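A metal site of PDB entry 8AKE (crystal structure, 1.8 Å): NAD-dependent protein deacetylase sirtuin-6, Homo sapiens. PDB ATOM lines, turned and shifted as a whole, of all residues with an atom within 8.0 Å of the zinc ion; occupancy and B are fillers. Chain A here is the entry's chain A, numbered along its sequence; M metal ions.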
ATOM      1  N   GLU A 134      -6.314 -28.959   4.165  1.00  0.00           N
ATOM      2  CA  GLU A 134      -6.241 -29.195   2.702  1.00  0.00           C
ATOM      3  C   GLU A 134      -5.298 -28.161   2.075  1.00  0.00           C
ATOM      4  O   GLU A 134      -5.434 -26.972   2.425  1.00  0.00           O
ATOM      5  CB  GLU A 134      -7.629 -29.103   2.065  1.00  0.00           C
ATOM      6  CG  GLU A 134      -7.626 -29.470   0.580  1.00  0.00           C
ATOM      7  CD  GLU A 134      -8.962 -29.654  -0.095  1.00  0.00           C
ATOM      8  OE1 GLU A 134      -9.876 -30.277   0.511  1.00  0.00           O
ATOM      9  OE2 GLU A 134      -9.080 -29.216  -1.267  1.00  0.00           O
ATOM     10  N   CYS A 135      -4.401 -28.629   1.195  1.00  0.00           N
ATOM     11  CA  CYS A 135      -3.482 -27.784   0.380  1.00  0.00           C
ATOM     12  C   CYS A 135      -4.281 -27.090  -0.719  1.00  0.00           C
ATOM     13  O   CYS A 135      -4.869 -27.798  -1.565  1.00  0.00           O
ATOM     14  CB  CYS A 135      -2.347 -28.585  -0.261  1.00  0.00           C
ATOM     15  SG  CYS A 135      -1.287 -27.591  -1.342  1.00  0.00           S
ATOM     16  N   ALA A 136      -4.297 -25.752  -0.686  1.00  0.00           N
ATOM     17  CA  ALA A 136      -4.980 -24.862  -1.652  1.00  0.00           C
ATOM     18  C   ALA A 136      -4.452 -25.107  -3.076  1.00  0.00           C
ATOM     19  O   ALA A 136      -5.262 -25.038  -4.017  1.00  0.00           O
ATOM     20  CB  ALA A 136      -4.772 -23.432  -1.241  1.00  0.00           C
ATOM     21  N   LYS A 137      -3.145 -25.394  -3.208  1.00  0.00           N
ATOM     22  CA  LYS A 137      -2.477 -25.586  -4.519  1.00  0.00           C
ATOM     23  C   LYS A 137      -2.828 -26.969  -5.119  1.00  0.00           C
ATOM     24  O   LYS A 137      -3.381 -26.975  -6.238  1.00  0.00           O
ATOM     25  CB  LYS A 137      -0.958 -25.406  -4.384  1.00  0.00           C
ATOM     26  CG  LYS A 137      -0.557 -24.050  -3.815  1.00  0.00           C
ATOM     27  CD  LYS A 137       0.645 -23.403  -4.470  1.00  0.00           C
ATOM     28  CE  LYS A 137       0.798 -21.947  -4.058  1.00  0.00           C
ATOM     29  NZ  LYS A 137       1.813 -21.238  -4.874  1.00  0.00           N
ATOM     30  N   CYS A 138      -2.522 -28.063  -4.431  1.00  0.00           N
ATOM     31  CA  CYS A 138      -2.606 -29.458  -4.984  1.00  0.00           C
ATOM     32  C   CYS A 138      -3.829 -30.216  -4.433  1.00  0.00           C
ATOM     33  O   CYS A 138      -4.034 -31.364  -4.890  1.00  0.00           O
ATOM     34  CB  CYS A 138      -1.313 -30.246  -4.777  1.00  0.00           C
ATOM     35  SG  CYS A 138      -0.899 -30.670  -3.054  1.00  0.00           S
ATOM     36  N   LYS A 139      -4.605 -29.630  -3.526  1.00  0.00           N
ATOM     37  CA  LYS A 139      -5.862 -30.215  -2.965  1.00  0.00           C
ATOM     38  C   LYS A 139      -5.561 -31.495  -2.163  1.00  0.00           C
ATOM     39  O   LYS A 139      -6.512 -32.303  -1.960  1.00  0.00           O
ATOM     40  CB  LYS A 139      -6.875 -30.532  -4.067  1.00  0.00           C
ATOM     41  CG  LYS A 139      -7.184 -29.391  -5.022  1.00  0.00           C
ATOM     42  CD  LYS A 139      -7.856 -28.212  -4.359  1.00  0.00           C
ATOM     43  CE  LYS A 139      -7.831 -26.967  -5.227  1.00  0.00           C
ATOM     44  NZ  LYS A 139      -8.272 -25.772  -4.477  1.00  0.00           N
ATOM     45  N   THR A 140      -4.310 -31.695  -1.737  1.00  0.00           N
ATOM     46  CA  THR A 140      -3.906 -32.852  -0.895  1.00  0.00           C
ATOM     47  C   THR A 140      -4.448 -32.586   0.515  1.00  0.00           C
ATOM     48  O   THR A 140      -4.262 -31.480   1.034  1.00  0.00           O
ATOM     49  CB  THR A 140      -2.391 -33.084  -0.917  1.00  0.00           C
ATOM     50  OG1 THR A 140      -2.036 -33.643  -2.171  1.00  0.00           O
ATOM     51  CG2 THR A 140      -1.895 -34.018   0.171  1.00  0.00           C
ATOM     52  N   GLN A 141      -5.108 -33.583   1.098  1.00  0.00           N
ATOM     53  CA  GLN A 141      -5.716 -33.498   2.449  1.00  0.00           C
ATOM     54  C   GLN A 141      -4.824 -34.241   3.437  1.00  0.00           C
ATOM     55  O   GLN A 141      -4.225 -35.285   3.043  1.00  0.00           O
ATOM     56  CB  GLN A 141      -7.118 -34.077   2.457  1.00  0.00           C
ATOM     57  CG  GLN A 141      -8.131 -33.166   1.834  1.00  0.00           C
ATOM     58  CD  GLN A 141      -9.513 -33.747   1.902  1.00  0.00           C
ATOM     59  OE1 GLN A 141      -9.700 -34.965   1.861  1.00  0.00           O
ATOM     60  NE2 GLN A 141     -10.512 -32.882   2.004  1.00  0.00           N
ATOM     61  N   TYR A 142      -4.699 -33.664   4.622  1.00  0.00           N
ATOM     62  CA  TYR A 142      -3.836 -34.164   5.730  1.00  0.00           C
ATOM     63  C   TYR A 142      -4.780 -34.405   6.892  1.00  0.00           C
ATOM     64  O   TYR A 142      -5.474 -33.450   7.275  1.00  0.00           O
ATOM     65  CB  TYR A 142      -2.763 -33.150   6.131  1.00  0.00           C
ATOM     66  CG  TYR A 142      -1.738 -32.839   5.078  1.00  0.00           C
ATOM     67  CD1 TYR A 142      -2.036 -31.993   4.019  1.00  0.00           C
ATOM     68  CD2 TYR A 142      -0.461 -33.377   5.138  1.00  0.00           C
ATOM     69  CE1 TYR A 142      -1.097 -31.708   3.047  1.00  0.00           C
ATOM     70  CE2 TYR A 142       0.492 -33.089   4.176  1.00  0.00           C
ATOM     71  CZ  TYR A 142       0.167 -32.256   3.125  1.00  0.00           C
ATOM     72  OH  TYR A 142       1.097 -31.949   2.170  1.00  0.00           O
ATOM     73  N   LEU A 159       2.500 -25.654   5.832  1.00  0.00           N
ATOM     74  CA  LEU A 159       2.647 -25.761   4.351  1.00  0.00           C
ATOM     75  C   LEU A 159       2.632 -27.221   3.921  1.00  0.00           C
ATOM     76  O   LEU A 159       2.863 -28.114   4.762  1.00  0.00           O
ATOM     77  CB  LEU A 159       3.935 -25.052   3.917  1.00  0.00           C
ATOM     78  CG  LEU A 159       3.959 -23.549   4.160  1.00  0.00           C
ATOM     79  CD1 LEU A 159       5.277 -22.957   3.682  1.00  0.00           C
ATOM     80  CD2 LEU A 159       2.789 -22.859   3.494  1.00  0.00           C
ATOM     81  N   CYS A 160       2.304 -27.441   2.648  1.00  0.00           N
ATOM     82  CA  CYS A 160       2.225 -28.751   1.973  1.00  0.00           C
ATOM     83  C   CYS A 160       3.628 -29.358   1.852  1.00  0.00           C
ATOM     84  O   CYS A 160       4.560 -28.589   1.567  1.00  0.00           O
ATOM     85  CB  CYS A 160       1.638 -28.605   0.586  1.00  0.00           C
ATOM     86  SG  CYS A 160       1.044 -30.149  -0.130  1.00  0.00           S
ATOM     87  N   THR A 161       3.748 -30.667   2.041  1.00  0.00           N
ATOM     88  CA  THR A 161       5.029 -31.415   2.073  1.00  0.00           C
ATOM     89  C   THR A 161       5.053 -32.464   0.946  1.00  0.00           C
ATOM     90  O   THR A 161       5.932 -33.336   1.004  1.00  0.00           O
ATOM     91  CB  THR A 161       5.269 -32.013   3.464  1.00  0.00           C
ATOM     92  OG1 THR A 161       4.258 -32.961   3.797  1.00  0.00           O
ATOM     93  CG2 THR A 161       5.267 -30.952   4.551  1.00  0.00           C
ATOM     94  N   VAL A 162       4.147 -32.376  -0.026  1.00  0.00           N
ATOM     95  CA  VAL A 162       4.095 -33.293  -1.216  1.00  0.00           C
ATOM     96  C   VAL A 162       5.389 -33.096  -2.012  1.00  0.00           C
ATOM     97  O   VAL A 162       5.673 -31.938  -2.356  1.00  0.00           O
ATOM     98  CB  VAL A 162       2.861 -33.031  -2.093  1.00  0.00           C
ATOM     99  CG1 VAL A 162       2.913 -33.846  -3.384  1.00  0.00           C
ATOM    100  CG2 VAL A 162       1.563 -33.290  -1.357  1.00  0.00           C
ATOM    101  N   ALA A 163       6.088 -34.202  -2.302  1.00  0.00           N
ATOM    102  CA  ALA A 163       7.476 -34.279  -2.825  1.00  0.00           C
ATOM    103  C   ALA A 163       7.776 -33.093  -3.744  1.00  0.00           C
ATOM    104  O   ALA A 163       7.662 -33.267  -4.973  1.00  0.00           O
ATOM    105  CB  ALA A 163       7.697 -35.598  -3.527  1.00  0.00           C
ATOM    106  N   CYS A 171       5.943 -28.585  -2.822  1.00  0.00           N
ATOM    107  CA  CYS A 171       4.688 -27.857  -3.172  1.00  0.00           C
ATOM    108  C   CYS A 171       4.585 -26.571  -2.339  1.00  0.00           C
ATOM    109  O   CYS A 171       4.227 -25.519  -2.901  1.00  0.00           O
ATOM    110  CB  CYS A 171       3.474 -28.753  -2.940  1.00  0.00           C
ATOM    111  SG  CYS A 171       1.910 -27.941  -3.316  1.00  0.00           S
ATOM    112  N   ARG A 172       4.885 -26.683  -1.044  1.00  0.00           N
ATOM    113  CA  ARG A 172       4.873 -25.583  -0.049  1.00  0.00           C
ATOM    114  C   ARG A 172       3.566 -24.812  -0.167  1.00  0.00           C
ATOM    115  O   ARG A 172       3.562 -23.614   0.169  1.00  0.00           O
ATOM    116  CB  ARG A 172       6.093 -24.655  -0.200  1.00  0.00           C
ATOM    117  CG  ARG A 172       7.434 -25.342  -0.029  1.00  0.00           C
ATOM    118  CD  ARG A 172       8.432 -24.538   0.794  1.00  0.00           C
ATOM    119  NE  ARG A 172       8.306 -23.092   0.613  1.00  0.00           N
ATOM    120  CZ  ARG A 172       8.195 -22.191   1.588  1.00  0.00           C
ATOM    121  NH1 ARG A 172       8.214 -22.561   2.855  1.00  0.00           N
ATOM    122  NH2 ARG A 172       8.076 -20.910   1.287  1.00  0.00           N
ATOM    123  N   GLY A 173       2.502 -25.478  -0.615  1.00  0.00           N
ATOM    124  CA  GLY A 173       1.141 -24.910  -0.726  1.00  0.00           C
ATOM    125  C   GLY A 173       0.602 -24.543   0.640  1.00  0.00           C
ATOM    126  O   GLY A 173       0.923 -25.254   1.621  1.00  0.00           O
ATOM    127  N   GLU A 174      -0.132 -23.433   0.715  1.00  0.00           N
ATOM    128  CA  GLU A 174      -0.902 -23.030   1.924  1.00  0.00           C
ATOM    129  C   GLU A 174      -1.849 -24.180   2.301  1.00  0.00           C
ATOM    130  O   GLU A 174      -2.676 -24.567   1.441  1.00  0.00           O
ATOM    131  CB  GLU A 174      -1.649 -21.728   1.627  1.00  0.00           C
ATOM    132  CG  GLU A 174      -2.135 -20.974   2.849  1.00  0.00           C
ATOM    133  CD  GLU A 174      -2.520 -19.541   2.530  1.00  0.00           C
ATOM    134  OE1 GLU A 174      -1.701 -18.860   1.872  1.00  0.00           O
ATOM    135  OE2 GLU A 174      -3.630 -19.094   2.915  1.00  0.00           O
ATOM    136  N   LEU A 175      -1.715 -24.745   3.498  1.00  0.00           N
ATOM    137  CA  LEU A 175      -2.715 -25.680   4.063  1.00  0.00           C
ATOM    138  C   LEU A 175      -3.844 -24.832   4.686  1.00  0.00           C
ATOM    139  O   LEU A 175      -3.523 -23.771   5.269  1.00  0.00           O
ATOM    140  CB  LEU A 175      -2.090 -26.606   5.105  1.00  0.00           C
ATOM    141  CG  LEU A 175      -0.897 -27.453   4.666  1.00  0.00           C
ATOM    142  CD1 LEU A 175      -0.558 -28.454   5.773  1.00  0.00           C
ATOM    143  CD2 LEU A 175      -1.154 -28.186   3.360  1.00  0.00           C
HETATM  144 ZN    ZN M   1       0.221 -29.199  -2.092  1.00  0.00          ZN
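OG1 of Thr 140 lies close to SG of Cys 138 (3.3 Å).
The backbone NH (N) of Gly 173 lies close to the side-chain sulfur (SG) of Cys 171 (3.7 Å).
The side-chain hydroxyl (OH) of Tyr 142 lies close to the side-chain sulfur (SG) of Cys 160 (2.9 Å).
The backbone carbonyl oxygen (O) of Val 162 sits at hydrogen-bond distance from the backbone NH (N) of Cys 171 (3.4 Å).
The backbone NH (N) of Cys 135 is in hydrogen-bond range of the backbone carbonyl oxygen (O) of Thr 140.
The backbone NH of Arg 172 is in hydrogen-bond range of the backbone carbonyl oxygen of Cys 160 (3.2 Å).
N of Lys 137 lies close to SG of Cys 135 (3.4 Å).
The backbone NH (N) of Cys 160 is in hydrogen-bond range of the backbone carbonyl oxygen (O) of Gly 173 (2.8 Å).
Within 4 Å of the zinc ion: Cys 135, Cys 138, Cys 160 and Cys 171.
SG of Cys 138 is bound to the zinc ion.
SG of Cys 135 binds the zinc ion, 2.3 Å away.
The side-chain sulfur (SG) of Cys 160 binds the zinc ion (2.3 Å).
SG of Cys 171 binds the zinc ion (2.4 Å).
The zinc ion has four donor atoms within binding distance.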
